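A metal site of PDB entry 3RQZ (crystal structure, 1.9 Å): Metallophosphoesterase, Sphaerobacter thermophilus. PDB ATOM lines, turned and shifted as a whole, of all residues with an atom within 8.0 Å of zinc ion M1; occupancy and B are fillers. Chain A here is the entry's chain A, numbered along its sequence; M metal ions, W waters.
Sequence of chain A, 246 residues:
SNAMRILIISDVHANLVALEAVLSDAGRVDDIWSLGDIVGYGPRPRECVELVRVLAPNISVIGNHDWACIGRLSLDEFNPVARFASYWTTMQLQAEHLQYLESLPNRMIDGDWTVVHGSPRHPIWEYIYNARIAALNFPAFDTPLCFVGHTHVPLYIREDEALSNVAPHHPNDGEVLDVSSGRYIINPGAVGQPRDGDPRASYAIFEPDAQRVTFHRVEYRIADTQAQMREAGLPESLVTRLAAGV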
ATOM      1  N   SER A  10     -23.379  18.266  33.025  1.00  0.00           N
ATOM      2  CA  SER A  10     -22.644  18.101  31.789  1.00  0.00           C
ATOM      3  C   SER A  10     -23.396  18.755  30.655  1.00  0.00           C
ATOM      4  O   SER A  10     -24.637  18.902  30.714  1.00  0.00           O
ATOM      5  CB  SER A  10     -22.442  16.603  31.494  1.00  0.00           C
ATOM      6  OG  SER A  10     -21.527  16.412  30.432  1.00  0.00           O
ATOM      7  N   ASP A  11     -22.659  19.156  29.622  1.00  0.00           N
ATOM      8  CA  ASP A  11     -23.260  19.550  28.345  1.00  0.00           C
ATOM      9  C   ASP A  11     -24.240  20.705  28.522  1.00  0.00           C
ATOM     10  O   ASP A  11     -25.379  20.689  28.017  1.00  0.00           O
ATOM     11  CB  ASP A  11     -23.849  18.313  27.618  1.00  0.00           C
ATOM     12  CG  ASP A  11     -22.794  17.232  27.343  1.00  0.00           C
ATOM     13  OD1 ASP A  11     -21.995  17.403  26.383  1.00  0.00           O
ATOM     14  OD2 ASP A  11     -22.748  16.225  28.091  1.00  0.00           O
ATOM     15  N   VAL A  12     -23.791  21.705  29.260  1.00  0.00           N
ATOM     16  CA  VAL A  12     -24.523  22.956  29.409  1.00  0.00           C
ATOM     17  C   VAL A  12     -24.728  23.621  28.032  1.00  0.00           C
ATOM     18  O   VAL A  12     -25.819  24.122  27.722  1.00  0.00           O
ATOM     19  CB  VAL A  12     -23.794  23.879  30.407  1.00  0.00           C
ATOM     20  CG1 VAL A  12     -24.444  25.286  30.413  1.00  0.00           C
ATOM     21  CG2 VAL A  12     -23.800  23.224  31.819  1.00  0.00           C
ATOM     22  N   HIS A  13     -23.698  23.595  27.192  1.00  0.00           N
ATOM     23  CA  HIS A  13     -23.854  24.071  25.838  1.00  0.00           C
ATOM     24  C   HIS A  13     -24.464  25.459  25.787  1.00  0.00           C
ATOM     25  O   HIS A  13     -25.431  25.697  25.063  1.00  0.00           O
ATOM     26  CB  HIS A  13     -24.636  23.054  24.966  1.00  0.00           C
ATOM     27  CG  HIS A  13     -23.778  21.912  24.493  1.00  0.00           C
ATOM     28  ND1 HIS A  13     -22.621  22.106  23.766  1.00  0.00           N
ATOM     29  CD2 HIS A  13     -23.888  20.569  24.676  1.00  0.00           C
ATOM     30  CE1 HIS A  13     -22.069  20.922  23.504  1.00  0.00           C
ATOM     31  NE2 HIS A  13     -22.818  19.980  24.049  1.00  0.00           N
ATOM     32  N   LEU A  35     -18.766  18.285  33.640  1.00  0.00           N
ATOM     33  CA  LEU A  35     -18.162  17.331  32.734  1.00  0.00           C
ATOM     34  C   LEU A  35     -17.915  17.895  31.337  1.00  0.00           C
ATOM     35  O   LEU A  35     -17.666  17.143  30.399  1.00  0.00           O
ATOM     36  CB  LEU A  35     -19.033  16.055  32.689  1.00  0.00           C
ATOM     37  CG  LEU A  35     -18.854  15.044  33.821  1.00  0.00           C
ATOM     38  CD1 LEU A  35     -18.902  15.681  35.216  1.00  0.00           C
ATOM     39  CD2 LEU A  35     -19.897  13.850  33.706  1.00  0.00           C
ATOM     40  N   GLY A  36     -17.921  19.217  31.193  1.00  0.00           N
ATOM     41  CA  GLY A  36     -17.470  19.804  29.927  1.00  0.00           C
ATOM     42  C   GLY A  36     -18.595  20.087  28.958  1.00  0.00           C
ATOM     43  O   GLY A  36     -19.783  19.828  29.268  1.00  0.00           O
ATOM     44  N   ASP A  37     -18.211  20.584  27.776  1.00  0.00           N
ATOM     45  CA  ASP A  37     -19.169  21.165  26.834  1.00  0.00           C
ATOM     46  C   ASP A  37     -20.043  22.248  27.484  1.00  0.00           C
ATOM     47  O   ASP A  37     -21.272  22.227  27.425  1.00  0.00           O
ATOM     48  CB  ASP A  37     -20.035  20.080  26.156  1.00  0.00           C
ATOM     49  CG  ASP A  37     -19.337  19.429  24.979  1.00  0.00           C
ATOM     50  OD1 ASP A  37     -18.160  19.751  24.672  1.00  0.00           O
ATOM     51  OD2 ASP A  37     -19.953  18.564  24.344  1.00  0.00           O
ATOM     52  N   ILE A  38     -19.357  23.220  28.102  1.00  0.00           N
ATOM     53  CA  ILE A  38     -19.948  24.429  28.597  1.00  0.00           C
ATOM     54  C   ILE A  38     -20.468  25.322  27.453  1.00  0.00           C
ATOM     55  O   ILE A  38     -21.429  26.070  27.631  1.00  0.00           O
ATOM     56  CB  ILE A  38     -18.879  25.209  29.393  1.00  0.00           C
ATOM     57  CG1 ILE A  38     -18.179  24.279  30.403  1.00  0.00           C
ATOM     58  CG2 ILE A  38     -19.491  26.366  30.104  1.00  0.00           C
ATOM     59  CD1 ILE A  38     -16.969  24.929  31.161  1.00  0.00           C
ATOM     60  N   VAL A  39     -19.822  25.268  26.282  1.00  0.00           N
ATOM     61  CA  VAL A  39     -20.169  26.148  25.165  1.00  0.00           C
ATOM     62  C   VAL A  39     -20.545  25.305  23.974  1.00  0.00           C
ATOM     63  O   VAL A  39     -20.414  24.072  24.013  1.00  0.00           O
ATOM     64  CB  VAL A  39     -19.003  27.126  24.770  1.00  0.00           C
ATOM     65  CG1 VAL A  39     -18.559  28.010  25.973  1.00  0.00           C
ATOM     66  CG2 VAL A  39     -17.787  26.315  24.230  1.00  0.00           C
ATOM     67  N   GLY A  40     -20.962  25.971  22.902  1.00  0.00           N
ATOM     68  CA  GLY A  40     -21.380  25.316  21.664  1.00  0.00           C
ATOM     69  C   GLY A  40     -22.888  25.217  21.610  1.00  0.00           C
ATOM     70  O   GLY A  40     -23.519  24.931  22.634  1.00  0.00           O
ATOM     71  N   TYR A  41     -23.467  25.474  20.439  1.00  0.00           N
ATOM     72  CA  TYR A  41     -24.928  25.387  20.220  1.00  0.00           C
ATOM     73  C   TYR A  41     -25.750  26.531  20.829  1.00  0.00           C
ATOM     74  O   TYR A  41     -26.516  27.178  20.125  1.00  0.00           O
ATOM     75  CB  TYR A  41     -25.518  24.047  20.729  1.00  0.00           C
ATOM     76  CG  TYR A  41     -24.929  22.797  20.143  1.00  0.00           C
ATOM     77  CD1 TYR A  41     -24.770  22.653  18.762  1.00  0.00           C
ATOM     78  CD2 TYR A  41     -24.515  21.747  20.961  1.00  0.00           C
ATOM     79  CE1 TYR A  41     -24.235  21.505  18.212  1.00  0.00           C
ATOM     80  CE2 TYR A  41     -23.985  20.572  20.424  1.00  0.00           C
ATOM     81  CZ  TYR A  41     -23.850  20.476  19.055  1.00  0.00           C
ATOM     82  OH  TYR A  41     -23.316  19.343  18.495  1.00  0.00           O
ATOM     83  N   GLY A  63     -14.766  19.578  27.440  1.00  0.00           N
ATOM     84  CA  GLY A  63     -15.526  18.793  26.444  1.00  0.00           C
ATOM     85  C   GLY A  63     -14.996  19.032  25.030  1.00  0.00           C
ATOM     86  O   GLY A  63     -14.141  19.914  24.819  1.00  0.00           O
ATOM     87  N   ASN A  64     -15.500  18.263  24.051  1.00  0.00           N
ATOM     88  CA  ASN A  64     -15.021  18.431  22.674  1.00  0.00           C
ATOM     89  C   ASN A  64     -15.387  19.804  22.083  1.00  0.00           C
ATOM     90  O   ASN A  64     -14.607  20.408  21.307  1.00  0.00           O
ATOM     91  CB  ASN A  64     -15.525  17.277  21.775  1.00  0.00           C
ATOM     92  CG  ASN A  64     -17.041  17.085  21.846  1.00  0.00           C
ATOM     93  OD1 ASN A  64     -17.598  16.890  22.922  1.00  0.00           O
ATOM     94  ND2 ASN A  64     -17.712  17.107  20.690  1.00  0.00           N
ATOM     95  N   HIS A  65     -16.565  20.306  22.426  1.00  0.00           N
ATOM     96  CA  HIS A  65     -16.940  21.680  21.942  1.00  0.00           C
ATOM     97  C   HIS A  65     -16.080  22.795  22.541  1.00  0.00           C
ATOM     98  O   HIS A  65     -15.702  23.736  21.819  1.00  0.00           O
ATOM     99  CB  HIS A  65     -18.439  21.954  22.115  1.00  0.00           C
ATOM    100  CG  HIS A  65     -19.261  21.176  21.149  1.00  0.00           C
ATOM    101  ND1 HIS A  65     -19.760  21.730  19.995  1.00  0.00           N
ATOM    102  CD2 HIS A  65     -19.618  19.864  21.142  1.00  0.00           C
ATOM    103  CE1 HIS A  65     -20.409  20.796  19.313  1.00  0.00           C
ATOM    104  NE2 HIS A  65     -20.344  19.655  19.993  1.00  0.00           N
ATOM    105  N   ASP A  66     -15.788  22.709  23.846  1.00  0.00           N
ATOM    106  CA  ASP A  66     -14.851  23.651  24.487  1.00  0.00           C
ATOM    107  C   ASP A  66     -13.493  23.602  23.773  1.00  0.00           C
ATOM    108  O   ASP A  66     -12.923  24.648  23.464  1.00  0.00           O
ATOM    109  CB  ASP A  66     -14.642  23.363  26.000  1.00  0.00           C
ATOM    110  CG  ASP A  66     -15.932  23.043  26.734  1.00  0.00           C
ATOM    111  OD1 ASP A  66     -16.933  23.787  26.527  1.00  0.00           O
ATOM    112  OD2 ASP A  66     -15.955  22.039  27.520  1.00  0.00           O
ATOM    113  N   HIS A 117     -15.221  13.752  29.981  1.00  0.00           N
ATOM    114  CA  HIS A 117     -16.339  14.179  29.197  1.00  0.00           C
ATOM    115  C   HIS A 117     -16.955  13.002  28.426  1.00  0.00           C
ATOM    116  O   HIS A 117     -18.172  12.876  28.333  1.00  0.00           O
ATOM    117  CB  HIS A 117     -15.905  15.243  28.191  1.00  0.00           C
ATOM    118  CG  HIS A 117     -17.015  15.716  27.317  1.00  0.00           C
ATOM    119  ND1 HIS A 117     -18.085  16.427  27.824  1.00  0.00           N
ATOM    120  CD2 HIS A 117     -17.250  15.555  25.990  1.00  0.00           C
ATOM    121  CE1 HIS A 117     -18.925  16.695  26.844  1.00  0.00           C
ATOM    122  NE2 HIS A 117     -18.446  16.185  25.722  1.00  0.00           N
ATOM    123  N   TYR A 127     -18.136   8.252  22.823  1.00  0.00           N
ATOM    124  CA  TYR A 127     -19.481   8.129  23.431  1.00  0.00           C
ATOM    125  C   TYR A 127     -19.629   6.776  24.107  1.00  0.00           C
ATOM    126  O   TYR A 127     -19.173   5.769  23.571  1.00  0.00           O
ATOM    127  CB  TYR A 127     -20.606   8.265  22.399  1.00  0.00           C
ATOM    128  CG  TYR A 127     -20.637   9.555  21.614  1.00  0.00           C
ATOM    129  CD1 TYR A 127     -21.293  10.685  22.114  1.00  0.00           C
ATOM    130  CD2 TYR A 127     -20.053   9.630  20.353  1.00  0.00           C
ATOM    131  CE1 TYR A 127     -21.337  11.882  21.377  1.00  0.00           C
ATOM    132  CE2 TYR A 127     -20.081  10.800  19.605  1.00  0.00           C
ATOM    133  CZ  TYR A 127     -20.743  11.921  20.125  1.00  0.00           C
ATOM    134  OH  TYR A 127     -20.783  13.080  19.404  1.00  0.00           O
ATOM    135  N   GLY A 149     -20.121  12.271  30.253  1.00  0.00           N
ATOM    136  CA  GLY A 149     -21.217  13.023  29.600  1.00  0.00           C
ATOM    137  C   GLY A 149     -21.279  12.694  28.118  1.00  0.00           C
ATOM    138  O   GLY A 149     -21.278  11.486  27.744  1.00  0.00           O
ATOM    139  N   HIS A 150     -21.395  13.739  27.291  1.00  0.00           N
ATOM    140  CA  HIS A 150     -21.154  13.686  25.824  1.00  0.00           C
ATOM    141  C   HIS A 150     -22.343  13.109  25.016  1.00  0.00           C
ATOM    142  O   HIS A 150     -22.635  13.576  23.919  1.00  0.00           O
ATOM    143  CB  HIS A 150     -19.840  12.896  25.573  1.00  0.00           C
ATOM    144  CG  HIS A 150     -19.244  13.034  24.206  1.00  0.00           C
ATOM    145  ND1 HIS A 150     -19.399  14.136  23.396  1.00  0.00           N
ATOM    146  CD2 HIS A 150     -18.430  12.184  23.529  1.00  0.00           C
ATOM    147  CE1 HIS A 150     -18.728  13.960  22.268  1.00  0.00           C
ATOM    148  NE2 HIS A 150     -18.117  12.779  22.337  1.00  0.00           N
ATOM    149  N   THR A 151     -23.049  12.132  25.545  1.00  0.00           N
ATOM    150  CA  THR A 151     -24.186  11.592  24.815  1.00  0.00           C
ATOM    151  C   THR A 151     -25.441  12.468  24.959  1.00  0.00           C
ATOM    152  O   THR A 151     -26.338  12.407  24.129  1.00  0.00           O
ATOM    153  CB  THR A 151     -24.546  10.195  25.331  1.00  0.00           C
ATOM    154  OG1 THR A 151     -24.866  10.317  26.723  1.00  0.00           O
ATOM    155  CG2 THR A 151     -23.365   9.227  25.165  1.00  0.00           C
ATOM    156  N   HIS A 152     -25.507  13.249  26.039  1.00  0.00           N
ATOM    157  CA  HIS A 152     -26.687  14.098  26.371  1.00  0.00           C
ATOM    158  C   HIS A 152     -27.881  13.248  26.795  1.00  0.00           C
ATOM    159  O   HIS A 152     -29.084  13.652  26.669  1.00  0.00           O
ATOM    160  CB  HIS A 152     -27.089  15.025  25.209  1.00  0.00           C
ATOM    161  CG  HIS A 152     -26.015  15.964  24.767  1.00  0.00           C
ATOM    162  ND1 HIS A 152     -26.275  17.020  23.924  1.00  0.00           N
ATOM    163  CD2 HIS A 152     -24.678  15.995  25.004  1.00  0.00           C
ATOM    164  CE1 HIS A 152     -25.159  17.671  23.673  1.00  0.00           C
ATOM    165  NE2 HIS A 152     -24.173  17.064  24.299  1.00  0.00           N
ATOM    166  N   ALA A 190     -27.638  15.846  29.811  1.00  0.00           N
ATOM    167  CA  ALA A 190     -27.224  17.207  29.476  1.00  0.00           C
ATOM    168  C   ALA A 190     -28.105  18.214  30.157  1.00  0.00           C
ATOM    169  O   ALA A 190     -29.328  18.051  30.187  1.00  0.00           O
ATOM    170  CB  ALA A 190     -27.280  17.459  27.989  1.00  0.00           C
ATOM    171  N   GLN A 193     -28.842  20.574  26.313  1.00  0.00           N
ATOM    172  CA  GLN A 193     -29.337  20.074  25.027  1.00  0.00           C
ATOM    173  C   GLN A 193     -29.640  18.594  25.156  1.00  0.00           C
ATOM    174  O   GLN A 193     -28.912  17.756  24.604  1.00  0.00           O
ATOM    175  CB  GLN A 193     -28.312  20.336  23.888  1.00  0.00           C
ATOM    176  CG  GLN A 193     -28.930  20.227  22.495  1.00  0.00           C
ATOM    177  CD  GLN A 193     -27.905  19.872  21.423  1.00  0.00           C
ATOM    178  OE1 GLN A 193     -27.182  18.874  21.531  1.00  0.00           O
ATOM    179  NE2 GLN A 193     -27.832  20.699  20.406  1.00  0.00           N
ATOM    180  N   ARG A 195     -31.024  14.901  24.554  1.00  0.00           N
ATOM    181  CA  ARG A 195     -31.192  14.195  23.285  1.00  0.00           C
ATOM    182  C   ARG A 195     -32.017  12.912  23.454  1.00  0.00           C
ATOM    183  O   ARG A 195     -32.005  12.036  22.585  1.00  0.00           O
ATOM    184  CB  ARG A 195     -29.821  13.882  22.644  1.00  0.00           C
ATOM    185  CG  ARG A 195     -29.070  15.128  22.117  1.00  0.00           C
ATOM    186  CD  ARG A 195     -27.825  14.754  21.286  1.00  0.00           C
ATOM    187  NE  ARG A 195     -27.105  15.965  20.931  1.00  0.00           N
ATOM    188  CZ  ARG A 195     -26.036  16.030  20.138  1.00  0.00           C
ATOM    189  NH1 ARG A 195     -25.517  14.924  19.590  1.00  0.00           N
ATOM    190  NH2 ARG A 195     -25.478  17.227  19.911  1.00  0.00           N
HETATM  191 ZN    ZN M   1     -22.070  17.895  24.277  1.00  0.00          ZN
HETATM  192 ZN    ZN M   2     -20.468  16.158  23.458  1.00  0.00          ZN
HETATM  193  O   HOH W   1     -22.006  17.517  21.856  1.00  0.00           O
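O of His 152 sits at hydrogen-bond distance from N of Arg 195 (3.1 Å). N of His 150 is in hydrogen-bond range of OD2 of Asp 11 (2.9 Å). The backbone NH (N) of His 13 is in hydrogen-bond range of the backbone carbonyl oxygen (O) of Ile 38 (3.4 Å). The backbone NH (N) of Asp 37 is in hydrogen-bond range of the side-chain carboxylate (OD2) of Asp 66 (2.7 Å). A ring nitrogen (ND1) of His 13 is in hydrogen-bond range of the backbone carbonyl oxygen (O) of Val 39. The side-chain carboxylate (OD2) of Asp 11 is in hydrogen-bond range of the side-chain hydroxyl (OG) of Ser 10 (2.6 Å). The backbone carbonyl oxygen (O) of Gln 193 sits at hydrogen-bond distance from a ring nitrogen (ND1) of His 152 (2.8 Å). O of Gly 40 sits at hydrogen-bond distance from ND1 of His 13, 3.2 Å away.
Of the 24 residues printed, 4 come within 4 Å of zinc ion M1. The nearest printed residue that does not touch zinc ion M1 is His 117 (4.2 Å).
Zinc ion M1 is bound by OD1 of Asp 11. Zinc ion M1 is bound by OD2 of Asp 37. Zinc ion M1 is bound by NE2 of His 13 (2.2 Å). Zinc ion M1 is bound by NE2 of His 152. Zinc ion M1 is bound by water W1, 2.5 Å away. Zinc ion M1 has five donor atoms within binding distance.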
